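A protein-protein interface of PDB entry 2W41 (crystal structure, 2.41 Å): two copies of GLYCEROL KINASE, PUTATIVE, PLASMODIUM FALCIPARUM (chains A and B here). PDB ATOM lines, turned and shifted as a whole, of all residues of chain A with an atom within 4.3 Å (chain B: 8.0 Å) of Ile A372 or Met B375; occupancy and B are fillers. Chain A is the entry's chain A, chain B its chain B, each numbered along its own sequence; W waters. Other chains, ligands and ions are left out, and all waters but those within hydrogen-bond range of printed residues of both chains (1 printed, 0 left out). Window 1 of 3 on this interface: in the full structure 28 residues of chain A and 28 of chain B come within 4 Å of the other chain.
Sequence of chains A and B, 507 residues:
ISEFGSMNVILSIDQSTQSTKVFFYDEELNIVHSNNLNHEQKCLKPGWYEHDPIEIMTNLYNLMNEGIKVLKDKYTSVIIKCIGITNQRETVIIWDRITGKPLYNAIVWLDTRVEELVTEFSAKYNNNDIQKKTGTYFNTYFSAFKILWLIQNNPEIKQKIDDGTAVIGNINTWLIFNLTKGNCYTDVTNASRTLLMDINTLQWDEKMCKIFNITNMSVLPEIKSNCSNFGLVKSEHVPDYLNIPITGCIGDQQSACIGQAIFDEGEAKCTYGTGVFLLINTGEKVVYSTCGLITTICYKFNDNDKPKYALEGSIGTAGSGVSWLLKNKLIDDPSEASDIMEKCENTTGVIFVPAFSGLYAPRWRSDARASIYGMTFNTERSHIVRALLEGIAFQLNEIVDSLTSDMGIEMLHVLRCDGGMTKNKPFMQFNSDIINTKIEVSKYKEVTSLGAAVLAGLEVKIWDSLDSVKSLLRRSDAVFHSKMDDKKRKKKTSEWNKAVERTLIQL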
ATOM      1  N   TRP A 324      27.941 -24.170  -1.688  1.00  0.00           N
ATOM      2  CA  TRP A 324      26.931 -23.300  -1.070  1.00  0.00           C
ATOM      3  C   TRP A 324      25.531 -24.008  -0.932  1.00  0.00           C
ATOM      4  O   TRP A 324      24.839 -23.870   0.088  1.00  0.00           O
ATOM      5  CB  TRP A 324      26.873 -21.985  -1.852  1.00  0.00           C
ATOM      6  CG  TRP A 324      25.829 -20.998  -1.362  1.00  0.00           C
ATOM      7  CD1 TRP A 324      26.031 -19.947  -0.531  1.00  0.00           C
ATOM      8  CD2 TRP A 324      24.425 -20.992  -1.682  1.00  0.00           C
ATOM      9  NE1 TRP A 324      24.853 -19.281  -0.316  1.00  0.00           N
ATOM     10  CE2 TRP A 324      23.846 -19.914  -0.996  1.00  0.00           C
ATOM     11  CE3 TRP A 324      23.599 -21.803  -2.488  1.00  0.00           C
ATOM     12  CZ2 TRP A 324      22.477 -19.618  -1.074  1.00  0.00           C
ATOM     13  CZ3 TRP A 324      22.228 -21.503  -2.562  1.00  0.00           C
ATOM     14  CH2 TRP A 324      21.690 -20.424  -1.858  1.00  0.00           C
ATOM     15  N   VAL A 350      11.925 -21.933 -12.833  1.00  0.00           N
ATOM     16  CA  VAL A 350      12.866 -21.369 -11.867  1.00  0.00           C
ATOM     17  C   VAL A 350      14.219 -20.970 -12.496  1.00  0.00           C
ATOM     18  O   VAL A 350      14.832 -21.750 -13.220  1.00  0.00           O
ATOM     19  CB  VAL A 350      13.057 -22.325 -10.674  1.00  0.00           C
ATOM     20  CG1 VAL A 350      14.149 -21.815  -9.714  1.00  0.00           C
ATOM     21  CG2 VAL A 350      11.766 -22.454  -9.923  1.00  0.00           C
ATOM     22  N   ILE A 351      14.668 -19.740 -12.264  1.00  0.00           N
ATOM     23  CA  ILE A 351      16.008 -19.313 -12.778  1.00  0.00           C
ATOM     24  C   ILE A 351      16.874 -18.794 -11.658  1.00  0.00           C
ATOM     25  O   ILE A 351      16.395 -18.039 -10.842  1.00  0.00           O
ATOM     26  CB  ILE A 351      15.911 -18.276 -13.893  1.00  0.00           C
ATOM     27  CG1 ILE A 351      15.050 -18.811 -15.019  1.00  0.00           C
ATOM     28  CG2 ILE A 351      17.298 -17.868 -14.374  1.00  0.00           C
ATOM     29  CD1 ILE A 351      14.936 -17.912 -16.200  1.00  0.00           C
ATOM     30  N   PHE A 352      18.122 -19.262 -11.611  1.00  0.00           N
ATOM     31  CA  PHE A 352      19.121 -18.906 -10.592  1.00  0.00           C
ATOM     32  C   PHE A 352      20.255 -18.193 -11.331  1.00  0.00           C
ATOM     33  O   PHE A 352      20.961 -18.800 -12.209  1.00  0.00           O
ATOM     34  CB  PHE A 352      19.689 -20.177  -9.973  1.00  0.00           C
ATOM     35  CG  PHE A 352      20.203 -20.052  -8.558  1.00  0.00           C
ATOM     36  CD1 PHE A 352      19.886 -21.042  -7.621  1.00  0.00           C
ATOM     37  CD2 PHE A 352      21.035 -19.004  -8.152  1.00  0.00           C
ATOM     38  CE1 PHE A 352      20.378 -20.982  -6.274  1.00  0.00           C
ATOM     39  CE2 PHE A 352      21.539 -18.919  -6.827  1.00  0.00           C
ATOM     40  CZ  PHE A 352      21.214 -19.912  -5.890  1.00  0.00           C
ATOM     41  N   PHE A 356      27.285 -14.907  -7.055  1.00  0.00           N
ATOM     42  CA  PHE A 356      27.698 -14.702  -5.660  1.00  0.00           C
ATOM     43  C   PHE A 356      28.817 -13.647  -5.509  1.00  0.00           C
ATOM     44  O   PHE A 356      28.873 -12.958  -4.486  1.00  0.00           O
ATOM     45  CB  PHE A 356      28.135 -16.026  -5.013  1.00  0.00           C
ATOM     46  CG  PHE A 356      27.113 -17.174  -5.138  1.00  0.00           C
ATOM     47  CD1 PHE A 356      26.157 -17.381  -4.152  1.00  0.00           C
ATOM     48  CD2 PHE A 356      27.142 -18.062  -6.217  1.00  0.00           C
ATOM     49  CE1 PHE A 356      25.243 -18.407  -4.223  1.00  0.00           C
ATOM     50  CE2 PHE A 356      26.200 -19.119  -6.294  1.00  0.00           C
ATOM     51  CZ  PHE A 356      25.249 -19.271  -5.280  1.00  0.00           C
ATOM     52  N   ARG A 369      24.372  -9.700  -7.543  1.00  0.00           N
ATOM     53  CA  ARG A 369      24.328 -10.720  -6.489  1.00  0.00           C
ATOM     54  C   ARG A 369      23.541 -11.987  -6.891  1.00  0.00           C
ATOM     55  O   ARG A 369      22.794 -11.999  -7.908  1.00  0.00           O
ATOM     56  CB  ARG A 369      23.716 -10.113  -5.228  1.00  0.00           C
ATOM     57  CG  ARG A 369      24.398  -8.842  -4.754  1.00  0.00           C
ATOM     58  CD  ARG A 369      25.638  -9.292  -4.012  1.00  0.00           C
ATOM     59  NE  ARG A 369      26.420  -8.193  -3.533  1.00  0.00           N
ATOM     60  CZ  ARG A 369      27.502  -7.725  -4.149  1.00  0.00           C
ATOM     61  NH1 ARG A 369      27.921  -8.266  -5.296  1.00  0.00           N
ATOM     62  NH2 ARG A 369      28.167  -6.702  -3.604  1.00  0.00           N
ATOM     63  N   ALA A 370      23.651 -13.037  -6.066  1.00  0.00           N
ATOM     64  CA  ALA A 370      22.991 -14.288  -6.415  1.00  0.00           C
ATOM     65  C   ALA A 370      21.463 -14.160  -6.269  1.00  0.00           C
ATOM     66  O   ALA A 370      20.949 -13.660  -5.269  1.00  0.00           O
ATOM     67  CB  ALA A 370      23.592 -15.515  -5.688  1.00  0.00           C
ATOM     68  N   SER A 371      20.735 -14.548  -7.320  1.00  0.00           N
ATOM     69  CA  SER A 371      19.314 -14.261  -7.358  1.00  0.00           C
ATOM     70  C   SER A 371      18.535 -15.450  -7.905  1.00  0.00           C
ATOM     71  O   SER A 371      18.918 -16.030  -8.883  1.00  0.00           O
ATOM     72  CB  SER A 371      19.072 -12.978  -8.182  1.00  0.00           C
ATOM     73  OG  SER A 371      19.991 -11.952  -7.819  1.00  0.00           O
ATOM     74  N   ILE A 372      17.427 -15.787  -7.262  1.00  0.00           N
ATOM     75  CA  ILE A 372      16.579 -16.907  -7.698  1.00  0.00           C
ATOM     76  C   ILE A 372      15.201 -16.347  -7.960  1.00  0.00           C
ATOM     77  O   ILE A 372      14.711 -15.565  -7.171  1.00  0.00           O
ATOM     78  CB  ILE A 372      16.428 -18.009  -6.633  1.00  0.00           C
ATOM     79  CG1 ILE A 372      17.709 -18.181  -5.835  1.00  0.00           C
ATOM     80  CG2 ILE A 372      15.970 -19.322  -7.250  1.00  0.00           C
ATOM     81  CD1 ILE A 372      17.611 -19.244  -4.788  1.00  0.00           C
ATOM     82  N   TYR A 373      14.616 -16.773  -9.083  1.00  0.00           N
ATOM     83  CA  TYR A 373      13.383 -16.249  -9.624  1.00  0.00           C
ATOM     84  C   TYR A 373      12.459 -17.403  -9.990  1.00  0.00           C
ATOM     85  O   TYR A 373      12.918 -18.494 -10.365  1.00  0.00           O
ATOM     86  CB  TYR A 373      13.680 -15.505 -10.925  1.00  0.00           C
ATOM     87  CG  TYR A 373      14.631 -14.326 -10.821  1.00  0.00           C
ATOM     88  CD1 TYR A 373      14.171 -13.111 -10.380  1.00  0.00           C
ATOM     89  CD2 TYR A 373      15.984 -14.435 -11.197  1.00  0.00           C
ATOM     90  CE1 TYR A 373      14.984 -12.032 -10.289  1.00  0.00           C
ATOM     91  CE2 TYR A 373      16.838 -13.321 -11.116  1.00  0.00           C
ATOM     92  CZ  TYR A 373      16.307 -12.115 -10.649  1.00  0.00           C
ATOM     93  OH  TYR A 373      17.036 -10.958 -10.546  1.00  0.00           O
ATOM     94  N   MET A 375       9.895 -19.023  -8.378  1.00  0.00           N
ATOM     95  CA  MET A 375       9.459 -20.060  -7.446  1.00  0.00           C
ATOM     96  C   MET A 375       7.964 -19.974  -6.991  1.00  0.00           C
ATOM     97  O   MET A 375       7.378 -18.887  -6.900  1.00  0.00           O
ATOM     98  CB  MET A 375      10.366 -20.103  -6.215  1.00  0.00           C
ATOM     99  CG  MET A 375      11.850 -20.348  -6.451  1.00  0.00           C
ATOM    100  SD  MET A 375      12.839 -20.304  -4.928  1.00  0.00           S
ATOM    101  CE  MET A 375      12.522 -18.620  -4.303  1.00  0.00           C
ATOM    102  N   TRP B 324       7.532 -24.491   3.497  1.00  0.00           N
ATOM    103  CA  TRP B 324       8.402 -24.561   2.316  1.00  0.00           C
ATOM    104  C   TRP B 324       9.932 -24.524   2.676  1.00  0.00           C
ATOM    105  O   TRP B 324      10.754 -25.247   2.099  1.00  0.00           O
ATOM    106  CB  TRP B 324       7.994 -23.439   1.322  1.00  0.00           C
ATOM    107  CG  TRP B 324       8.790 -23.350   0.068  1.00  0.00           C
ATOM    108  CD1 TRP B 324       8.446 -23.839  -1.146  1.00  0.00           C
ATOM    109  CD2 TRP B 324      10.064 -22.703  -0.103  1.00  0.00           C
ATOM    110  NE1 TRP B 324       9.433 -23.571  -2.070  1.00  0.00           N
ATOM    111  CE2 TRP B 324      10.446 -22.879  -1.447  1.00  0.00           C
ATOM    112  CE3 TRP B 324      10.942 -22.004   0.762  1.00  0.00           C
ATOM    113  CZ2 TRP B 324      11.651 -22.385  -1.947  1.00  0.00           C
ATOM    114  CZ3 TRP B 324      12.169 -21.545   0.250  1.00  0.00           C
ATOM    115  CH2 TRP B 324      12.494 -21.719  -1.078  1.00  0.00           C
ATOM    116  N   THR B 347      19.743  -9.613   7.593  1.00  0.00           N
ATOM    117  CA  THR B 347      19.903 -10.608   6.519  1.00  0.00           C
ATOM    118  C   THR B 347      21.131 -10.281   5.623  1.00  0.00           C
ATOM    119  O   THR B 347      21.313 -10.861   4.570  1.00  0.00           O
ATOM    120  CB  THR B 347      18.642 -10.630   5.662  1.00  0.00           C
ATOM    121  OG1 THR B 347      18.432  -9.330   5.111  1.00  0.00           O
ATOM    122  CG2 THR B 347      17.453 -10.922   6.491  1.00  0.00           C
ATOM    123  N   THR B 348      21.970  -9.351   6.083  1.00  0.00           N
ATOM    124  CA  THR B 348      23.100  -8.803   5.332  1.00  0.00           C
ATOM    125  C   THR B 348      22.774  -8.484   3.854  1.00  0.00           C
ATOM    126  O   THR B 348      23.484  -8.910   2.954  1.00  0.00           O
ATOM    127  CB  THR B 348      24.441  -9.648   5.507  1.00  0.00           C
ATOM    128  OG1 THR B 348      24.456 -10.792   4.625  1.00  0.00           O
ATOM    129  CG2 THR B 348      24.658 -10.113   6.979  1.00  0.00           C
ATOM    130  N   GLY B 349      21.693  -7.727   3.632  1.00  0.00           N
ATOM    131  CA  GLY B 349      21.275  -7.288   2.299  1.00  0.00           C
ATOM    132  C   GLY B 349      20.366  -8.237   1.514  1.00  0.00           C
ATOM    133  O   GLY B 349      19.817  -7.831   0.489  1.00  0.00           O
ATOM    134  N   VAL B 350      20.210  -9.485   1.972  1.00  0.00           N
ATOM    135  CA  VAL B 350      19.321 -10.465   1.353  1.00  0.00           C
ATOM    136  C   VAL B 350      17.821 -10.101   1.458  1.00  0.00           C
ATOM    137  O   VAL B 350      17.325  -9.794   2.530  1.00  0.00           O
ATOM    138  CB  VAL B 350      19.605 -11.887   1.893  1.00  0.00           C
ATOM    139  CG1 VAL B 350      18.640 -12.928   1.283  1.00  0.00           C
ATOM    140  CG2 VAL B 350      21.010 -12.293   1.561  1.00  0.00           C
ATOM    141  N   ILE B 351      17.113 -10.099   0.330  1.00  0.00           N
ATOM    142  CA  ILE B 351      15.651  -9.857   0.328  1.00  0.00           C
ATOM    143  C   ILE B 351      14.901 -10.991  -0.349  1.00  0.00           C
ATOM    144  O   ILE B 351      15.288 -11.425  -1.425  1.00  0.00           O
ATOM    145  CB  ILE B 351      15.276  -8.523  -0.331  1.00  0.00           C
ATOM    146  CG1 ILE B 351      15.983  -7.379   0.390  1.00  0.00           C
ATOM    147  CG2 ILE B 351      13.772  -8.322  -0.362  1.00  0.00           C
ATOM    148  CD1 ILE B 351      15.684  -6.011  -0.160  1.00  0.00           C
ATOM    149  N   PHE B 352      13.832 -11.443   0.300  1.00  0.00           N
ATOM    150  CA  PHE B 352      12.966 -12.521  -0.184  1.00  0.00           C
ATOM    151  C   PHE B 352      11.574 -11.943  -0.421  1.00  0.00           C
ATOM    152  O   PHE B 352      10.902 -11.524   0.514  1.00  0.00           O
ATOM    153  CB  PHE B 352      12.843 -13.589   0.894  1.00  0.00           C
ATOM    154  CG  PHE B 352      12.631 -14.993   0.397  1.00  0.00           C
ATOM    155  CD1 PHE B 352      13.340 -16.054   0.992  1.00  0.00           C
ATOM    156  CD2 PHE B 352      11.680 -15.298  -0.581  1.00  0.00           C
ATOM    157  CE1 PHE B 352      13.092 -17.381   0.615  1.00  0.00           C
ATOM    158  CE2 PHE B 352      11.437 -16.615  -0.975  1.00  0.00           C
ATOM    159  CZ  PHE B 352      12.148 -17.660  -0.388  1.00  0.00           C
ATOM    160  N   VAL B 353      11.142 -11.914  -1.675  1.00  0.00           N
ATOM    161  CA  VAL B 353       9.769 -11.510  -1.985  1.00  0.00           C
ATOM    162  C   VAL B 353       9.009 -12.815  -2.024  1.00  0.00           C
ATOM    163  O   VAL B 353       9.092 -13.558  -2.986  1.00  0.00           O
ATOM    164  CB  VAL B 353       9.735 -10.754  -3.311  1.00  0.00           C
ATOM    165  CG1 VAL B 353       8.326 -10.375  -3.719  1.00  0.00           C
ATOM    166  CG2 VAL B 353      10.655  -9.476  -3.216  1.00  0.00           C
ATOM    167  N   ARG B 369       6.283 -14.182  -8.803  1.00  0.00           N
ATOM    168  CA  ARG B 369       6.763 -15.433  -8.182  1.00  0.00           C
ATOM    169  C   ARG B 369       7.766 -15.204  -7.050  1.00  0.00           C
ATOM    170  O   ARG B 369       8.301 -14.091  -6.887  1.00  0.00           O
ATOM    171  CB  ARG B 369       7.380 -16.364  -9.228  1.00  0.00           C
ATOM    172  CG  ARG B 369       6.499 -16.665 -10.412  1.00  0.00           C
ATOM    173  CD  ARG B 369       5.557 -17.725  -9.965  1.00  0.00           C
ATOM    174  NE  ARG B 369       4.641 -18.131 -11.003  1.00  0.00           N
ATOM    175  CZ  ARG B 369       3.405 -17.672 -11.130  1.00  0.00           C
ATOM    176  NH1 ARG B 369       2.923 -16.752 -10.301  1.00  0.00           N
ATOM    177  NH2 ARG B 369       2.651 -18.123 -12.123  1.00  0.00           N
ATOM    178  N   ALA B 370       8.051 -16.259  -6.295  1.00  0.00           N
ATOM    179  CA  ALA B 370       8.930 -16.126  -5.138  1.00  0.00           C
ATOM    180  C   ALA B 370      10.366 -15.851  -5.607  1.00  0.00           C
ATOM    181  O   ALA B 370      10.893 -16.530  -6.488  1.00  0.00           O
ATOM    182  CB  ALA B 370       8.817 -17.315  -4.158  1.00  0.00           C
ATOM    183  N   SER B 371      10.987 -14.820  -5.023  1.00  0.00           N
ATOM    184  CA  SER B 371      12.248 -14.339  -5.542  1.00  0.00           C
ATOM    185  C   SER B 371      13.169 -13.937  -4.422  1.00  0.00           C
ATOM    186  O   SER B 371      12.741 -13.302  -3.481  1.00  0.00           O
ATOM    187  CB  SER B 371      12.008 -13.173  -6.519  1.00  0.00           C
ATOM    188  OG  SER B 371      11.045 -13.497  -7.529  1.00  0.00           O
ATOM    189  N   ILE B 372      14.437 -14.289  -4.547  1.00  0.00           N
ATOM    190  CA  ILE B 372      15.428 -14.015  -3.490  1.00  0.00           C
ATOM    191  C   ILE B 372      16.571 -13.267  -4.116  1.00  0.00           C
ATOM    192  O   ILE B 372      17.011 -13.613  -5.193  1.00  0.00           O
ATOM    193  CB  ILE B 372      16.014 -15.278  -2.801  1.00  0.00           C
ATOM    194  CG1 ILE B 372      14.971 -16.377  -2.644  1.00  0.00           C
ATOM    195  CG2 ILE B 372      16.647 -14.907  -1.470  1.00  0.00           C
ATOM    196  CD1 ILE B 372      15.517 -17.694  -2.015  1.00  0.00           C
ATOM    197  N   TYR B 373      17.030 -12.229  -3.428  1.00  0.00           N
ATOM    198  CA  TYR B 373      17.968 -11.279  -3.979  1.00  0.00           C
ATOM    199  C   TYR B 373      19.110 -11.045  -2.993  1.00  0.00           C
ATOM    200  O   TYR B 373      18.951 -11.186  -1.772  1.00  0.00           O
ATOM    201  CB  TYR B 373      17.269  -9.940  -4.236  1.00  0.00           C
ATOM    202  CG  TYR B 373      16.094  -9.969  -5.204  1.00  0.00           C
ATOM    203  CD1 TYR B 373      16.317  -9.979  -6.560  1.00  0.00           C
ATOM    204  CD2 TYR B 373      14.752  -9.958  -4.746  1.00  0.00           C
ATOM    205  CE1 TYR B 373      15.297  -9.986  -7.446  1.00  0.00           C
ATOM    206  CE2 TYR B 373      13.704  -9.968  -5.646  1.00  0.00           C
ATOM    207  CZ  TYR B 373      13.996  -9.988  -7.004  1.00  0.00           C
ATOM    208  OH  TYR B 373      13.019  -9.977  -7.987  1.00  0.00           O
ATOM    209  N   GLY B 374      20.254 -10.659  -3.537  1.00  0.00           N
ATOM    210  CA  GLY B 374      21.333 -10.092  -2.745  1.00  0.00           C
ATOM    211  C   GLY B 374      22.240 -11.086  -2.059  1.00  0.00           C
ATOM    212  O   GLY B 374      22.991 -10.705  -1.151  1.00  0.00           O
ATOM    213  N   MET B 375      22.169 -12.357  -2.457  1.00  0.00           N
ATOM    214  CA  MET B 375      23.025 -13.383  -1.880  1.00  0.00           C
ATOM    215  C   MET B 375      24.507 -13.367  -2.377  1.00  0.00           C
ATOM    216  O   MET B 375      24.809 -12.980  -3.520  1.00  0.00           O
ATOM    217  CB  MET B 375      22.408 -14.758  -2.084  1.00  0.00           C
ATOM    218  CG  MET B 375      21.006 -14.937  -1.543  1.00  0.00           C
ATOM    219  SD  MET B 375      20.314 -16.580  -1.793  1.00  0.00           S
ATOM    220  CE  MET B 375      20.284 -16.726  -3.606  1.00  0.00           C
ATOM    221  N   THR B 376      25.416 -13.795  -1.493  1.00  0.00           N
ATOM    222  CA  THR B 376      26.860 -13.974  -1.756  1.00  0.00           C
ATOM    223  C   THR B 376      27.201 -15.366  -1.257  1.00  0.00           C
ATOM    224  O   THR B 376      26.294 -16.073  -0.788  1.00  0.00           O
ATOM    225  CB  THR B 376      27.716 -12.947  -0.995  1.00  0.00           C
ATOM    226  OG1 THR B 376      27.576 -13.170   0.420  1.00  0.00           O
ATOM    227  CG2 THR B 376      27.305 -11.538  -1.314  1.00  0.00           C
ATOM    228  N   PHE B 377      28.472 -15.787  -1.346  1.00  0.00           N
ATOM    229  CA  PHE B 377      28.886 -17.139  -0.858  1.00  0.00           C
ATOM    230  C   PHE B 377      28.738 -17.223   0.659  1.00  0.00           C
ATOM    231  O   PHE B 377      28.601 -18.304   1.237  1.00  0.00           O
ATOM    232  CB  PHE B 377      30.310 -17.497  -1.264  1.00  0.00           C
ATOM    233  CG  PHE B 377      30.448 -18.021  -2.697  1.00  0.00           C
ATOM    234  CD1 PHE B 377      29.757 -19.170  -3.119  1.00  0.00           C
ATOM    235  CD2 PHE B 377      31.292 -17.368  -3.621  1.00  0.00           C
ATOM    236  CE1 PHE B 377      29.888 -19.661  -4.432  1.00  0.00           C
ATOM    237  CE2 PHE B 377      31.432 -17.846  -4.934  1.00  0.00           C
ATOM    238  CZ  PHE B 377      30.728 -18.999  -5.341  1.00  0.00           C
ATOM    239  N   ASN B 378      28.720 -16.054   1.285  1.00  0.00           N
ATOM    240  CA  ASN B 378      28.544 -15.936   2.712  1.00  0.00           C
ATOM    241  C   ASN B 378      27.118 -16.143   3.279  1.00  0.00           C
ATOM    242  O   ASN B 378      26.960 -16.465   4.469  1.00  0.00           O
ATOM    243  CB  ASN B 378      29.096 -14.586   3.147  1.00  0.00           C
ATOM    244  CG  ASN B 378      29.406 -14.560   4.607  1.00  0.00           C
ATOM    245  OD1 ASN B 378      28.714 -13.871   5.377  1.00  0.00           O
ATOM    246  ND2 ASN B 378      30.402 -15.374   5.032  1.00  0.00           N
ATOM    247  N   THR B 379      26.093 -15.930   2.456  1.00  0.00           N
ATOM    248  CA  THR B 379      24.696 -16.231   2.793  1.00  0.00           C
ATOM    249  C   THR B 379      24.418 -17.677   3.291  1.00  0.00           C
ATOM    250  O   THR B 379      24.869 -18.665   2.686  1.00  0.00           O
ATOM    251  CB  THR B 379      23.746 -15.875   1.586  1.00  0.00           C
ATOM    252  OG1 THR B 379      23.989 -14.526   1.159  1.00  0.00           O
ATOM    253  CG2 THR B 379      22.274 -16.054   1.961  1.00  0.00           C
ATOM    254  N   GLU B 380      23.618 -17.771   4.364  1.00  0.00           N
ATOM    255  CA  GLU B 380      23.365 -19.006   5.090  1.00  0.00           C
ATOM    256  C   GLU B 380      21.861 -19.310   5.266  1.00  0.00           C
ATOM    257  O   GLU B 380      21.054 -18.434   5.072  1.00  0.00           O
ATOM    258  CB  GLU B 380      23.984 -18.841   6.469  1.00  0.00           C
ATOM    259  CG  GLU B 380      25.469 -18.957   6.496  1.00  0.00           C
ATOM    260  CD  GLU B 380      25.965 -19.329   7.892  1.00  0.00           C
ATOM    261  OE1 GLU B 380      25.087 -19.460   8.791  1.00  0.00           O
ATOM    262  OE2 GLU B 380      27.207 -19.516   8.053  1.00  0.00           O
ATOM    263  N   HIS B 383      19.942 -16.528   6.956  1.00  0.00           N
ATOM    264  CA  HIS B 383      19.720 -15.240   6.274  1.00  0.00           C
ATOM    265  C   HIS B 383      18.487 -15.312   5.382  1.00  0.00           C
ATOM    266  O   HIS B 383      17.770 -14.327   5.231  1.00  0.00           O
ATOM    267  CB  HIS B 383      20.898 -14.841   5.426  1.00  0.00           C
ATOM    268  CG  HIS B 383      22.177 -14.684   6.185  1.00  0.00           C
ATOM    269  ND1 HIS B 383      22.469 -13.564   6.932  1.00  0.00           N
ATOM    270  CD2 HIS B 383      23.256 -15.489   6.285  1.00  0.00           C
ATOM    271  CE1 HIS B 383      23.658 -13.701   7.485  1.00  0.00           C
ATOM    272  NE2 HIS B 383      24.157 -14.858   7.103  1.00  0.00           N
ATOM    273  N   ILE B 384      18.271 -16.494   4.800  1.00  0.00           N
ATOM    274  CA  ILE B 384      17.195 -16.766   3.841  1.00  0.00           C
ATOM    275  C   ILE B 384      15.872 -16.919   4.575  1.00  0.00           C
ATOM    276  O   ILE B 384      14.875 -16.412   4.102  1.00  0.00           O
ATOM    277  CB  ILE B 384      17.499 -18.076   3.068  1.00  0.00           C
ATOM    278  CG1 ILE B 384      18.640 -17.862   2.082  1.00  0.00           C
ATOM    279  CG2 ILE B 384      16.196 -18.714   2.446  1.00  0.00           C
ATOM    280  CD1 ILE B 384      19.274 -19.180   1.604  1.00  0.00           C
ATOM    281  N   ALA B 387      14.848 -13.539   5.944  1.00  0.00           N
ATOM    282  CA  ALA B 387      14.385 -12.762   4.797  1.00  0.00           C
ATOM    283  C   ALA B 387      12.940 -13.099   4.447  1.00  0.00           C
ATOM    284  O   ALA B 387      12.135 -12.211   4.265  1.00  0.00           O
ATOM    285  CB  ALA B 387      15.288 -12.978   3.591  1.00  0.00           C
ATOM    286  N   THR B 503      11.020  -7.969  -9.333  1.00  0.00           N
ATOM    287  CA  THR B 503      10.109  -9.097  -9.378  1.00  0.00           C
ATOM    288  C   THR B 503       8.963  -8.889 -10.425  1.00  0.00           C
ATOM    289  O   THR B 503       8.503  -9.851 -11.049  1.00  0.00           O
ATOM    290  CB  THR B 503       9.594  -9.333  -7.938  1.00  0.00           C
ATOM    291  OG1 THR B 503      10.716  -9.661  -7.098  1.00  0.00           O
ATOM    292  CG2 THR B 503       8.511 -10.392  -7.851  1.00  0.00           C
HETATM  293  O   HOH W   1      19.994  -8.970  -6.408  1.00  0.00           O
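The backbone NH (N) of Tyr B373 is in hydrogen-bond range of the backbone carbonyl oxygen (O) of Ile B351 (2.8 Å). N of Tyr A373 lies within hydrogen-bond range of O of Ile A351 (2.8 Å). OG1 of Thr B379 sits at hydrogen-bond distance from N of Thr B376 (3.1 Å). The backbone carbonyl oxygen of Ser B371 lies within hydrogen-bond range of the backbone NH of Val B353, 2.8 Å away.
Of the printed residues of chain B, Trp A324 touches Met B375, Thr B376, Phe B377 and Thr B379. Of the printed residues of chain B, Arg A369 touches Gly B374 (3.4 Å), Met B375 (3.5 Å) and Thr B376 (3.9 Å). Of the printed residues of chain A, Met B375 touches Trp A324 (3.8 Å), Phe A356 (3.99 Å), Arg A369 (3.5 Å), Ala A370 (2.8 Å) and Ile A372 (3.7 Å). The nearest printed residue of chain A that does not touch Met B375 is Phe A352 (4.03 Å). The nearest printed residue of chain A that does not touch Tyr B373 is Ser A371 (4.4 Å).
Among the printed residues, pairs that only touch across the chains: Trp A324 with Met B375 (3.8 Å), Trp A324 with Thr B376 (3.5 Å), Trp A324 with Phe B377 (3.5 Å), Phe A356 with Met B375 (3.99 Å), Phe A356 with Thr B376 (3.5 Å), Phe A356 with Phe B377 (3.6 Å), Arg A369 with Gly B374 (3.4 Å), Arg A369 with Met B375 (3.5 Å), Arg A369 with Thr B376 (3.9 Å), Ala A370 with Ile B372 (3.9 Å), Ala A370 with Tyr B373 (3.9 Å), Ala A370 with Gly B374 (3.5 Å), Ser A371 with Ile B372 (3.2 Å), Ile A372 with Ala B370 (3.997 Å), Ile A372 with Ser B371 (3.2 Å), Ile A372 with Met B375 (3.7 Å), Tyr A373 with Ala B370 (3.9 Å), Tyr A373 with Tyr B373 (3.5 Å), Met A375 with Trp B324 (3.8 Å), Met A375 with Arg B369 (3.4 Å) and Met A375 with Ile B372 (3.7 Å).
Printed residues of chain A that touch a printed residue of chain B: Trp A324, Phe A356, Arg A369, Ala A370, Ser A371, Ile A372, Tyr A373 and Met A375. Printed residues of chain B that touch a printed residue of chain A: Trp B324, Arg B369, Ala B370, Ser B371, Ile B372, Tyr B373, Gly B374, Met B375, Thr B376, Phe B377 and Thr B379. Hydrophobic or aromatic side chains of chain B within 4 Å of the printed part of chain A: Trp B324, Ala B370, Ile B372, Tyr B373, Met B375 and Phe B377. Along chain B the printed residues that touch a printed residue of chain A span positions 324 to 379. Among the printed residues, no Asp or Glu carboxylate lies within 4 Å of a Lys or Arg side-chain nitrogen of the other chain.
Ala A370 touches Ile B372, and with the chains exchanged Ile A372 touches Ala B370. Ala A370 touches Tyr B373, and with the chains exchanged Tyr A373 touches Ala B370. Ile A372 touches Met B375, and with the chains exchanged Met A375 touches Ile B372. Positions printed for both chains: 324, 350, 351, 352, 369, 370, 371, 372, 373 and 375.
Water W1 lies within hydrogen-bond range of the side-chain hydroxyl of Ser A371 (3.3 Å) and the backbone NH of Gly B374 (3.3 Å).
The indole nitrogen of Trp A324 is in hydrogen-bond range of the backbone carbonyl oxygen of Thr B379 (3.1 Å). The backbone NH of Ala B370 is in hydrogen-bond range of the backbone carbonyl oxygen of Met A375 (2.8 Å). O of Ile A372 is in hydrogen-bond range of N of Ile B372 (2.9 Å). The backbone carbonyl oxygen of Met B375 lies within hydrogen-bond range of the backbone NH of Ala A370, at 2.8 Å.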
